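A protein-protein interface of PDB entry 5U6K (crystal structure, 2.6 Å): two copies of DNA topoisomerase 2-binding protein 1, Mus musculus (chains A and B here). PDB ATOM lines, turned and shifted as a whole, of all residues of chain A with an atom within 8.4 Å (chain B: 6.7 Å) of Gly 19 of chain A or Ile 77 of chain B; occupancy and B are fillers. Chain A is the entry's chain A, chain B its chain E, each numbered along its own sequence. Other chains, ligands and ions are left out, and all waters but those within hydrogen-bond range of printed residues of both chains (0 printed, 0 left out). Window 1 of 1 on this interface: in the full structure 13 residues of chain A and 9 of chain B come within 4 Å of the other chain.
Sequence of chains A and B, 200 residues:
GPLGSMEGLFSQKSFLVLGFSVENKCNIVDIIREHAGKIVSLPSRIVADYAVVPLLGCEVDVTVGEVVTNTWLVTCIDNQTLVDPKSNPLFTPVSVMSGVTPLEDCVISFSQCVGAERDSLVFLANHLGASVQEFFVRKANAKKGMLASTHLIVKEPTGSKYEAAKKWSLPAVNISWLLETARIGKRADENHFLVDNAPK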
ATOM      1  N   LEU A  16      30.186  10.131 -11.310  1.00  0.00           N
ATOM      2  CA  LEU A  16      30.244  10.902 -12.541  1.00  0.00           C
ATOM      3  C   LEU A  16      29.541  10.087 -13.612  1.00  0.00           C
ATOM      4  O   LEU A  16      29.683   8.862 -13.664  1.00  0.00           O
ATOM      5  CB  LEU A  16      31.680  11.173 -12.999  1.00  0.00           C
ATOM      6  CG  LEU A  16      32.591  12.106 -12.218  1.00  0.00           C
ATOM      7  CD1 LEU A  16      33.965  12.108 -12.869  1.00  0.00           C
ATOM      8  CD2 LEU A  16      32.003  13.502 -12.214  1.00  0.00           C
ATOM      9  N   VAL A  17      28.787  10.763 -14.462  1.00  0.00           N
ATOM     10  CA  VAL A  17      28.087  10.121 -15.564  1.00  0.00           C
ATOM     11  C   VAL A  17      28.631  10.738 -16.844  1.00  0.00           C
ATOM     12  O   VAL A  17      28.462  11.941 -17.082  1.00  0.00           O
ATOM     13  CB  VAL A  17      26.569  10.290 -15.453  1.00  0.00           C
ATOM     14  CG1 VAL A  17      25.872   9.540 -16.564  1.00  0.00           C
ATOM     15  CG2 VAL A  17      26.093   9.814 -14.079  1.00  0.00           C
ATOM     16  N   LEU A  18      29.314   9.924 -17.651  1.00  0.00           N
ATOM     17  CA  LEU A  18      30.023  10.393 -18.833  1.00  0.00           C
ATOM     18  C   LEU A  18      29.694   9.534 -20.043  1.00  0.00           C
ATOM     19  O   LEU A  18      29.453   8.325 -19.926  1.00  0.00           O
ATOM     20  CB  LEU A  18      31.552  10.390 -18.637  1.00  0.00           C
ATOM     21  CG  LEU A  18      32.100  11.110 -17.407  1.00  0.00           C
ATOM     22  CD1 LEU A  18      33.617  10.926 -17.311  1.00  0.00           C
ATOM     23  CD2 LEU A  18      31.713  12.587 -17.447  1.00  0.00           C
ATOM     24  N   GLY A  19      29.701  10.180 -21.211  1.00  0.00           N
ATOM     25  CA  GLY A  19      29.639   9.492 -22.482  1.00  0.00           C
ATOM     26  C   GLY A  19      28.255   9.160 -22.986  1.00  0.00           C
ATOM     27  O   GLY A  19      28.138   8.473 -24.009  1.00  0.00           O
ATOM     28  N   PHE A  20      27.204   9.614 -22.312  1.00  0.00           N
ATOM     29  CA  PHE A  20      25.838   9.311 -22.717  1.00  0.00           C
ATOM     30  C   PHE A  20      25.187  10.516 -23.387  1.00  0.00           C
ATOM     31  O   PHE A  20      25.672  11.647 -23.301  1.00  0.00           O
ATOM     32  CB  PHE A  20      25.003   8.876 -21.513  1.00  0.00           C
ATOM     33  CG  PHE A  20      25.489   7.623 -20.871  1.00  0.00           C
ATOM     34  CD1 PHE A  20      25.127   6.384 -21.373  1.00  0.00           C
ATOM     35  CD2 PHE A  20      26.304   7.681 -19.747  1.00  0.00           C
ATOM     36  CE1 PHE A  20      25.576   5.217 -20.766  1.00  0.00           C
ATOM     37  CE2 PHE A  20      26.758   6.523 -19.142  1.00  0.00           C
ATOM     38  CZ  PHE A  20      26.394   5.290 -19.658  1.00  0.00           C
ATOM     39  N   SER A  21      24.085  10.252 -24.084  1.00  0.00           N
ATOM     40  CA  SER A  21      23.290  11.332 -24.646  1.00  0.00           C
ATOM     41  C   SER A  21      22.526  12.051 -23.535  1.00  0.00           C
ATOM     42  O   SER A  21      22.487  11.606 -22.385  1.00  0.00           O
ATOM     43  CB  SER A  21      22.324  10.796 -25.705  1.00  0.00           C
ATOM     44  OG  SER A  21      21.378   9.902 -25.140  1.00  0.00           O
ATOM     45  N   VAL A  22      21.879  13.157 -23.906  1.00  0.00           N
ATOM     46  CA  VAL A  22      21.158  13.974 -22.931  1.00  0.00           C
ATOM     47  C   VAL A  22      20.068  13.165 -22.238  1.00  0.00           C
ATOM     48  O   VAL A  22      19.895  13.257 -21.015  1.00  0.00           O
ATOM     49  CB  VAL A  22      20.603  15.246 -23.608  1.00  0.00           C
ATOM     50  CG1 VAL A  22      19.650  15.993 -22.691  1.00  0.00           C
ATOM     51  CG2 VAL A  22      21.759  16.160 -23.983  1.00  0.00           C
ATOM     52  N   ASN A  24      19.724   9.739 -21.983  1.00  0.00           N
ATOM     53  CA  ASN A  24      20.253   8.635 -21.187  1.00  0.00           C
ATOM     54  C   ASN A  24      20.928   9.144 -19.921  1.00  0.00           C
ATOM     55  O   ASN A  24      20.864   8.490 -18.873  1.00  0.00           O
ATOM     56  CB  ASN A  24      21.230   7.793 -22.010  1.00  0.00           C
ATOM     57  CG  ASN A  24      20.539   6.989 -23.085  1.00  0.00           C
ATOM     58  OD1 ASN A  24      19.430   6.487 -22.876  1.00  0.00           O
ATOM     59  ND2 ASN A  24      21.182   6.869 -24.252  1.00  0.00           N
ATOM     60  N   LYS A  25      21.596  10.297 -20.003  1.00  0.00           N
ATOM     61  CA  LYS A  25      22.250  10.843 -18.821  1.00  0.00           C
ATOM     62  C   LYS A  25      21.231  11.180 -17.739  1.00  0.00           C
ATOM     63  O   LYS A  25      21.469  10.931 -16.555  1.00  0.00           O
ATOM     64  CB  LYS A  25      23.071  12.073 -19.189  1.00  0.00           C
ATOM     65  CG  LYS A  25      23.767  12.704 -18.009  1.00  0.00           C
ATOM     66  CD  LYS A  25      24.526  13.939 -18.432  1.00  0.00           C
ATOM     67  CE  LYS A  25      25.327  14.532 -17.289  1.00  0.00           C
ATOM     68  NZ  LYS A  25      26.069  15.753 -17.711  1.00  0.00           N
ATOM     69  N   ILE A  28      20.056   7.986 -16.045  1.00  0.00           N
ATOM     70  CA  ILE A  28      21.099   7.462 -15.170  1.00  0.00           C
ATOM     71  C   ILE A  28      21.261   8.352 -13.940  1.00  0.00           C
ATOM     72  O   ILE A  28      21.483   7.864 -12.823  1.00  0.00           O
ATOM     73  CB  ILE A  28      22.407   7.302 -15.970  1.00  0.00           C
ATOM     74  CG1 ILE A  28      22.262   6.141 -16.962  1.00  0.00           C
ATOM     75  CG2 ILE A  28      23.587   7.069 -15.051  1.00  0.00           C
ATOM     76  CD1 ILE A  28      23.384   6.031 -17.990  1.00  0.00           C
ATOM     77  N   VAL A  52      30.400   6.412 -14.255  1.00  0.00           N
ATOM     78  CA  VAL A  52      29.548   5.533 -15.050  1.00  0.00           C
ATOM     79  C   VAL A  52      29.711   5.893 -16.525  1.00  0.00           C
ATOM     80  O   VAL A  52      29.408   7.019 -16.935  1.00  0.00           O
ATOM     81  CB  VAL A  52      28.084   5.670 -14.614  1.00  0.00           C
ATOM     82  CG1 VAL A  52      27.219   4.616 -15.296  1.00  0.00           C
ATOM     83  CG2 VAL A  52      27.981   5.618 -13.089  1.00  0.00           C
ATOM     84  N   VAL A  53      30.159   4.935 -17.331  1.00  0.00           N
ATOM     85  CA  VAL A  53      30.430   5.179 -18.747  1.00  0.00           C
ATOM     86  C   VAL A  53      29.712   4.132 -19.598  1.00  0.00           C
ATOM     87  O   VAL A  53      29.230   3.127 -19.062  1.00  0.00           O
ATOM     88  CB  VAL A  53      31.943   5.170 -19.041  1.00  0.00           C
ATOM     89  CG1 VAL A  53      32.688   6.179 -18.162  1.00  0.00           C
ATOM     90  CG2 VAL A  53      32.512   3.758 -18.924  1.00  0.00           C
ATOM     91  N   PRO A  54      29.576   4.331 -20.910  1.00  0.00           N
ATOM     92  CA  PRO A  54      28.965   3.294 -21.753  1.00  0.00           C
ATOM     93  C   PRO A  54      29.789   2.012 -21.758  1.00  0.00           C
ATOM     94  O   PRO A  54      30.964   1.984 -21.378  1.00  0.00           O
ATOM     95  CB  PRO A  54      28.928   3.943 -23.136  1.00  0.00           C
ATOM     96  CG  PRO A  54      28.929   5.389 -22.863  1.00  0.00           C
ATOM     97  CD  PRO A  54      29.787   5.581 -21.661  1.00  0.00           C
ATOM     98  N   LEU A  55      29.166   0.942 -22.262  1.00  0.00           N
ATOM     99  CA  LEU A  55      29.801  -0.373 -22.228  1.00  0.00           C
ATOM    100  C   LEU A  55      31.158  -0.367 -22.923  1.00  0.00           C
ATOM    101  O   LEU A  55      32.122  -0.954 -22.412  1.00  0.00           O
ATOM    102  CB  LEU A  55      28.884  -1.414 -22.868  1.00  0.00           C
ATOM    103  CG  LEU A  55      29.434  -2.842 -22.876  1.00  0.00           C
ATOM    104  CD1 LEU A  55      29.589  -3.369 -21.453  1.00  0.00           C
ATOM    105  CD2 LEU A  55      28.470  -3.740 -23.658  1.00  0.00           C
ATOM    106  N   LEU A  56      31.260   0.288 -24.087  1.00  0.00           N
ATOM    107  CA  LEU A  56      32.555   0.375 -24.755  1.00  0.00           C
ATOM    108  C   LEU A  56      33.414   1.515 -24.230  1.00  0.00           C
ATOM    109  O   LEU A  56      34.516   1.725 -24.750  1.00  0.00           O
ATOM    110  CB  LEU A  56      32.393   0.514 -26.266  1.00  0.00           C
ATOM    111  CG  LEU A  56      31.577  -0.579 -26.965  1.00  0.00           C
ATOM    112  CD1 LEU A  56      31.819  -0.532 -28.467  1.00  0.00           C
ATOM    113  CD2 LEU A  56      31.798  -1.964 -26.374  1.00  0.00           C
ATOM    114  N   GLY A  57      32.949   2.240 -23.213  1.00  0.00           N
ATOM    115  CA  GLY A  57      33.750   3.276 -22.600  1.00  0.00           C
ATOM    116  C   GLY A  57      33.670   4.614 -23.309  1.00  0.00           C
ATOM    117  O   GLY A  57      32.999   4.798 -24.328  1.00  0.00           O
ATOM    118  N   CYS A  58      34.373   5.578 -22.724  1.00  0.00           N
ATOM    119  CA  CYS A  58      34.461   6.917 -23.273  1.00  0.00           C
ATOM    120  C   CYS A  58      35.707   7.579 -22.703  1.00  0.00           C
ATOM    121  O   CYS A  58      36.495   6.960 -21.987  1.00  0.00           O
ATOM    122  CB  CYS A  58      33.200   7.728 -22.975  1.00  0.00           C
ATOM    123  SG  CYS A  58      32.955   8.198 -21.265  1.00  0.00           S
ATOM    124  N   GLU A  59      35.896   8.841 -23.061  1.00  0.00           N
ATOM    125  CA  GLU A  59      37.042   9.601 -22.591  1.00  0.00           C
ATOM    126  C   GLU A  59      36.804  10.000 -21.139  1.00  0.00           C
ATOM    127  O   GLU A  59      35.778  10.608 -20.820  1.00  0.00           O
ATOM    128  CB  GLU A  59      37.250  10.828 -23.478  1.00  0.00           C
ATOM    129  CG  GLU A  59      38.553  11.576 -23.242  1.00  0.00           C
ATOM    130  CD  GLU A  59      39.768  10.825 -23.761  1.00  0.00           C
ATOM    131  OE1 GLU A  59      39.593   9.882 -24.565  1.00  0.00           O
ATOM    132  OE2 GLU A  59      40.899  11.179 -23.361  1.00  0.00           O
ATOM    133  N   VAL A  60      37.728   9.629 -20.255  1.00  0.00           N
ATOM    134  CA  VAL A  60      37.672  10.003 -18.846  1.00  0.00           C
ATOM    135  C   VAL A  60      38.973  10.727 -18.539  1.00  0.00           C
ATOM    136  O   VAL A  60      40.032  10.094 -18.438  1.00  0.00           O
ATOM    137  CB  VAL A  60      37.486   8.790 -17.925  1.00  0.00           C
ATOM    138  CG1 VAL A  60      37.329   9.244 -16.488  1.00  0.00           C
ATOM    139  CG2 VAL A  60      36.284   7.946 -18.366  1.00  0.00           C
ATOM    140  N   PHE A 123      24.052  -6.636 -27.146  1.00  0.00           N
ATOM    141  CA  PHE A 123      24.637  -5.453 -27.768  1.00  0.00           C
ATOM    142  C   PHE A 123      25.984  -5.777 -28.405  1.00  0.00           C
ATOM    143  O   PHE A 123      26.237  -5.421 -29.563  1.00  0.00           O
ATOM    144  CB  PHE A 123      24.773  -4.342 -26.727  1.00  0.00           C
ATOM    145  CG  PHE A 123      25.351  -3.071 -27.264  1.00  0.00           C
ATOM    146  CD1 PHE A 123      24.526  -2.083 -27.787  1.00  0.00           C
ATOM    147  CD2 PHE A 123      26.723  -2.851 -27.228  1.00  0.00           C
ATOM    148  CE1 PHE A 123      25.060  -0.899 -28.275  1.00  0.00           C
ATOM    149  CE2 PHE A 123      27.261  -1.676 -27.726  1.00  0.00           C
ATOM    150  CZ  PHE A 123      26.427  -0.696 -28.248  1.00  0.00           C
ATOM    151  N   LEU B   9      35.661   7.112 -30.091  1.00  0.00           N
ATOM    152  CA  LEU B   9      34.723   7.026 -31.208  1.00  0.00           C
ATOM    153  C   LEU B   9      35.004   8.093 -32.264  1.00  0.00           C
ATOM    154  O   LEU B   9      35.100   7.791 -33.460  1.00  0.00           O
ATOM    155  CB  LEU B   9      33.299   7.167 -30.672  1.00  0.00           C
ATOM    156  CG  LEU B   9      32.113   7.084 -31.620  1.00  0.00           C
ATOM    157  CD1 LEU B   9      32.056   5.703 -32.255  1.00  0.00           C
ATOM    158  CD2 LEU B   9      30.824   7.415 -30.883  1.00  0.00           C
ATOM    159  N   PHE B  10      35.119   9.351 -31.843  1.00  0.00           N
ATOM    160  CA  PHE B  10      35.408  10.460 -32.742  1.00  0.00           C
ATOM    161  C   PHE B  10      36.882  10.823 -32.746  1.00  0.00           C
ATOM    162  O   PHE B  10      37.236  11.955 -33.090  1.00  0.00           O
ATOM    163  CB  PHE B  10      34.571  11.682 -32.362  1.00  0.00           C
ATOM    164  CG  PHE B  10      33.102  11.439 -32.422  1.00  0.00           C
ATOM    165  CD1 PHE B  10      32.549  10.729 -33.471  1.00  0.00           C
ATOM    166  CD2 PHE B  10      32.274  11.906 -31.424  1.00  0.00           C
ATOM    167  CE1 PHE B  10      31.190  10.500 -33.533  1.00  0.00           C
ATOM    168  CE2 PHE B  10      30.914  11.677 -31.471  1.00  0.00           C
ATOM    169  CZ  PHE B  10      30.370  10.968 -32.526  1.00  0.00           C
ATOM    170  N   ILE B  31      29.246  16.364 -25.427  1.00  0.00           N
ATOM    171  CA  ILE B  31      29.048  15.025 -25.956  1.00  0.00           C
ATOM    172  C   ILE B  31      30.176  14.659 -26.919  1.00  0.00           C
ATOM    173  O   ILE B  31      30.723  13.553 -26.863  1.00  0.00           O
ATOM    174  CB  ILE B  31      27.662  14.955 -26.623  1.00  0.00           C
ATOM    175  CG1 ILE B  31      26.582  14.615 -25.591  1.00  0.00           C
ATOM    176  CG2 ILE B  31      27.661  13.983 -27.732  1.00  0.00           C
ATOM    177  CD1 ILE B  31      25.178  14.593 -26.166  1.00  0.00           C
ATOM    178  N   ILE B  32      30.572  15.598 -27.785  1.00  0.00           N
ATOM    179  CA  ILE B  32      31.639  15.317 -28.745  1.00  0.00           C
ATOM    180  C   ILE B  32      32.973  15.111 -28.030  1.00  0.00           C
ATOM    181  O   ILE B  32      33.726  14.183 -28.348  1.00  0.00           O
ATOM    182  CB  ILE B  32      31.717  16.447 -29.787  1.00  0.00           C
ATOM    183  CG1 ILE B  32      30.494  16.385 -30.701  1.00  0.00           C
ATOM    184  CG2 ILE B  32      33.009  16.354 -30.600  1.00  0.00           C
ATOM    185  CD1 ILE B  32      30.393  17.536 -31.673  1.00  0.00           C
ATOM    186  N   GLU B  34      33.517  14.146 -24.938  1.00  0.00           N
ATOM    187  CA  GLU B  34      33.518  12.921 -24.149  1.00  0.00           C
ATOM    188  C   GLU B  34      33.842  11.691 -24.983  1.00  0.00           C
ATOM    189  O   GLU B  34      34.128  10.631 -24.410  1.00  0.00           O
ATOM    190  CB  GLU B  34      32.163  12.738 -23.457  1.00  0.00           C
ATOM    191  CG  GLU B  34      31.934  13.694 -22.296  1.00  0.00           C
ATOM    192  CD  GLU B  34      30.532  13.609 -21.706  1.00  0.00           C
ATOM    193  OE1 GLU B  34      29.760  12.706 -22.085  1.00  0.00           O
ATOM    194  OE2 GLU B  34      30.205  14.452 -20.849  1.00  0.00           O
ATOM    195  N   HIS B  35      33.823  11.803 -26.314  1.00  0.00           N
ATOM    196  CA  HIS B  35      34.157  10.685 -27.184  1.00  0.00           C
ATOM    197  C   HIS B  35      35.388  10.990 -28.027  1.00  0.00           C
ATOM    198  O   HIS B  35      35.527  10.483 -29.145  1.00  0.00           O
ATOM    199  CB  HIS B  35      32.960  10.314 -28.056  1.00  0.00           C
ATOM    200  CG  HIS B  35      31.825   9.710 -27.287  1.00  0.00           C
ATOM    201  ND1 HIS B  35      31.758   8.365 -26.991  1.00  0.00           N
ATOM    202  CD2 HIS B  35      30.724  10.271 -26.735  1.00  0.00           C
ATOM    203  CE1 HIS B  35      30.656   8.121 -26.303  1.00  0.00           C
ATOM    204  NE2 HIS B  35      30.013   9.262 -26.130  1.00  0.00           N
ATOM    205  N   TRP B  72      22.412  12.079 -36.391  1.00  0.00           N
ATOM    206  CA  TRP B  72      23.554  11.208 -36.660  1.00  0.00           C
ATOM    207  C   TRP B  72      24.488  11.128 -35.461  1.00  0.00           C
ATOM    208  O   TRP B  72      25.007  10.055 -35.138  1.00  0.00           O
ATOM    209  CB  TRP B  72      24.313  11.704 -37.887  1.00  0.00           C
ATOM    210  CG  TRP B  72      25.655  11.057 -38.085  1.00  0.00           C
ATOM    211  CD1 TRP B  72      25.909   9.858 -38.692  1.00  0.00           C
ATOM    212  CD2 TRP B  72      26.932  11.601 -37.727  1.00  0.00           C
ATOM    213  NE1 TRP B  72      27.260   9.615 -38.717  1.00  0.00           N
ATOM    214  CE2 TRP B  72      27.912  10.669 -38.133  1.00  0.00           C
ATOM    215  CE3 TRP B  72      27.342  12.778 -37.092  1.00  0.00           C
ATOM    216  CZ2 TRP B  72      29.273  10.876 -37.923  1.00  0.00           C
ATOM    217  CZ3 TRP B  72      28.698  12.985 -36.885  1.00  0.00           C
ATOM    218  CH2 TRP B  72      29.647  12.037 -37.300  1.00  0.00           C
ATOM    219  N   LEU B  73      24.734  12.261 -34.813  1.00  0.00           N
ATOM    220  CA  LEU B  73      25.654  12.291 -33.688  1.00  0.00           C
ATOM    221  C   LEU B  73      25.141  11.420 -32.552  1.00  0.00           C
ATOM    222  O   LEU B  73      25.856  10.538 -32.056  1.00  0.00           O
ATOM    223  CB  LEU B  73      25.856  13.742 -33.244  1.00  0.00           C
ATOM    224  CG  LEU B  73      26.908  13.995 -32.166  1.00  0.00           C
ATOM    225  CD1 LEU B  73      28.299  13.759 -32.746  1.00  0.00           C
ATOM    226  CD2 LEU B  73      26.774  15.401 -31.632  1.00  0.00           C
ATOM    227  N   VAL B  74      23.887  11.635 -32.142  1.00  0.00           N
ATOM    228  CA  VAL B  74      23.325  10.857 -31.041  1.00  0.00           C
ATOM    229  C   VAL B  74      23.215   9.383 -31.416  1.00  0.00           C
ATOM    230  O   VAL B  74      23.398   8.506 -30.566  1.00  0.00           O
ATOM    231  CB  VAL B  74      21.964  11.445 -30.619  1.00  0.00           C
ATOM    232  CG1 VAL B  74      21.303  10.560 -29.574  1.00  0.00           C
ATOM    233  CG2 VAL B  74      22.149  12.852 -30.068  1.00  0.00           C
ATOM    234  N   THR B  75      22.929   9.081 -32.685  1.00  0.00           N
ATOM    235  CA  THR B  75      22.856   7.686 -33.110  1.00  0.00           C
ATOM    236  C   THR B  75      24.216   7.007 -33.007  1.00  0.00           C
ATOM    237  O   THR B  75      24.297   5.820 -32.674  1.00  0.00           O
ATOM    238  CB  THR B  75      22.313   7.588 -34.535  1.00  0.00           C
ATOM    239  OG1 THR B  75      21.008   8.175 -34.586  1.00  0.00           O
ATOM    240  CG2 THR B  75      22.214   6.135 -34.964  1.00  0.00           C
ATOM    241  N   CYS B  76      25.291   7.739 -33.296  1.00  0.00           N
ATOM    242  CA  CYS B  76      26.626   7.174 -33.132  1.00  0.00           C
ATOM    243  C   CYS B  76      26.905   6.867 -31.668  1.00  0.00           C
ATOM    244  O   CYS B  76      27.501   5.839 -31.338  1.00  0.00           O
ATOM    245  CB  CYS B  76      27.677   8.139 -33.681  1.00  0.00           C
ATOM    246  SG  CYS B  76      27.699   8.314 -35.483  1.00  0.00           S
ATOM    247  N   ILE B  77      26.491   7.762 -30.777  1.00  0.00           N
ATOM    248  CA  ILE B  77      26.746   7.592 -29.355  1.00  0.00           C
ATOM    249  C   ILE B  77      25.837   6.533 -28.750  1.00  0.00           C
ATOM    250  O   ILE B  77      26.294   5.693 -27.970  1.00  0.00           O
ATOM    251  CB  ILE B  77      26.601   8.953 -28.665  1.00  0.00           C
ATOM    252  CG1 ILE B  77      27.783   9.814 -29.090  1.00  0.00           C
ATOM    253  CG2 ILE B  77      26.554   8.803 -27.160  1.00  0.00           C
ATOM    254  CD1 ILE B  77      27.418  11.198 -29.358  1.00  0.00           C
ATOM    255  N   ASP B  78      24.549   6.524 -29.117  1.00  0.00           N
ATOM    256  CA  ASP B  78      23.646   5.517 -28.568  1.00  0.00           C
ATOM    257  C   ASP B  78      24.042   4.112 -29.004  1.00  0.00           C
ATOM    258  O   ASP B  78      23.781   3.144 -28.278  1.00  0.00           O
ATOM    259  CB  ASP B  78      22.202   5.783 -28.993  1.00  0.00           C
ATOM    260  CG  ASP B  78      21.650   7.073 -28.436  1.00  0.00           C
ATOM    261  OD1 ASP B  78      22.178   7.570 -27.422  1.00  0.00           O
ATOM    262  OD2 ASP B  78      20.666   7.586 -29.016  1.00  0.00           O
ATOM    263  N   ASN B  79      24.671   3.979 -30.173  1.00  0.00           N
ATOM    264  CA  ASN B  79      25.114   2.694 -30.697  1.00  0.00           C
ATOM    265  C   ASN B  79      26.612   2.489 -30.551  1.00  0.00           C
ATOM    266  O   ASN B  79      27.122   1.445 -30.970  1.00  0.00           O
ATOM    267  CB  ASN B  79      24.731   2.553 -32.171  1.00  0.00           C
ATOM    268  CG  ASN B  79      23.233   2.545 -32.384  1.00  0.00           C
ATOM    269  OD1 ASN B  79      22.471   2.104 -31.520  1.00  0.00           O
ATOM    270  ND2 ASN B  79      22.800   3.016 -33.550  1.00  0.00           N
ATOM    271  N   GLN B  80      27.329   3.486 -30.030  1.00  0.00           N
ATOM    272  CA  GLN B  80      28.768   3.378 -29.785  1.00  0.00           C
ATOM    273  C   GLN B  80      29.519   2.946 -31.044  1.00  0.00           C
ATOM    274  O   GLN B  80      30.450   2.138 -30.998  1.00  0.00           O
ATOM    275  CB  GLN B  80      29.038   2.429 -28.621  1.00  0.00           C
ATOM    276  CG  GLN B  80      28.251   2.784 -27.362  1.00  0.00           C
ATOM    277  CD  GLN B  80      28.309   1.678 -26.347  1.00  0.00           C
ATOM    278  OE1 GLN B  80      28.936   0.661 -26.576  1.00  0.00           O
ATOM    279  NE2 GLN B  80      27.637   1.852 -25.242  1.00  0.00           N
ATOM    280  N   THR B  81      29.096   3.489 -32.184  1.00  0.00           N
ATOM    281  CA  THR B  81      29.659   3.137 -33.478  1.00  0.00           C
ATOM    282  C   THR B  81      29.609   4.358 -34.381  1.00  0.00           C
ATOM    283  O   THR B  81      28.604   5.072 -34.400  1.00  0.00           O
ATOM    284  CB  THR B  81      28.886   1.985 -34.130  1.00  0.00           C
ATOM    285  OG1 THR B  81      28.782   0.895 -33.208  1.00  0.00           O
ATOM    286  CG2 THR B  81      29.602   1.510 -35.389  1.00  0.00           C
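No position is printed for both chains.
The backbone NH (N) of Phe 10 of chain B is in hydrogen-bond range of the backbone carbonyl oxygen (O) of His 35 of chain B, at 3.0 Å. ND2 of Asn 24 of chain A is in hydrogen-bond range of OG of Ser 21 of chain A. N of Leu 18 of chain A sits at hydrogen-bond distance from O of Val 52 of chain A. The backbone carbonyl oxygen (O) of Asn 79 of chain B sits at hydrogen-bond distance from the side-chain hydroxyl (OG1) of Thr 81 of chain B (2.8 Å). The side-chain amide nitrogen (ND2) of Asn 79 of chain B sits at hydrogen-bond distance from the backbone carbonyl oxygen (O) of Thr 75 of chain B, at 3.3 Å. The backbone carbonyl oxygen (O) of Leu 18 of chain A sits close to the side-chain sulfur (SG) of Cys 58 of chain A (3.8 Å).
Among the printed residues, merely in contact across the chains: Phe 123 of chain A with Gln 80 of chain B, Pro 54 of chain A with Gln 80 of chain B, Cys 58 of chain A with Glu 34 of chain B, Phe 123 of chain A with Asn 79 of chain B, Gly 19 of chain A with Ile 77 of chain B, Leu 18 of chain A with Glu 34 of chain B and Phe 20 of chain A with Ile 31 of chain B.
Of chain B, only Glu 34 (2.7 Å), His 35 (2.9 Å) and Ile 77 (3.5 Å) come within 4 Å of Gly 19 of chain A. Printed residues of chain B within 4 Å of Phe 20 of chain A: Ile 31. Printed residues of chain B within 4 Å of Asn 24 of chain A: Asp 78. Of the printed residues of chain B, Glu 59 of chain A touches Glu 34 (2.9 Å). Of the printed residues of chain A, His 35 of chain B touches Gly 19 (2.9 Å). Leu 73 of chain B touches none of the printed residues of chain A. Ile 77 of chain B touches just one residue of chain A: Gly 19.
Hydrophobic or aromatic side chains of chain A that line the printed part of chain B: Pro 54, Leu 56 and Phe 123. Among the printed residues, 14 pairs touch across the chains. Among the printed residues, no Asp or Glu carboxylate lies within 4 Å of a Lys or Arg side-chain nitrogen of the other chain.
The side-chain hydroxyl (OG) of Ser 21 of chain A lies within hydrogen-bond range of the side-chain carboxylate (OD1) of Asp 78 of chain B. The backbone NH (N) of Leu 56 of chain A lies close to the side-chain amide oxygen (OE1) of Gln 80 of chain B (3.4 Å). The side-chain amide nitrogen of Asn 24 of chain A lies within hydrogen-bond range of the side-chain carboxylate of Asp 78 of chain B, 3.4 Å away. N of Leu 55 of chain A sits close to NE2 of Gln 80 of chain B, 3.5 Å away. O of Gly 19 of chain A lies within hydrogen-bond range of NE2 of His 35 of chain B, 2.9 Å away. The backbone NH of Glu 59 of chain A sits at hydrogen-bond distance from the backbone carbonyl oxygen of Glu 34 of chain B, 2.9 Å away. The backbone NH (N) of Gly 19 of chain A is in hydrogen-bond range of the side-chain carboxylate (OE1) of Glu 34 of chain B (2.7 Å).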
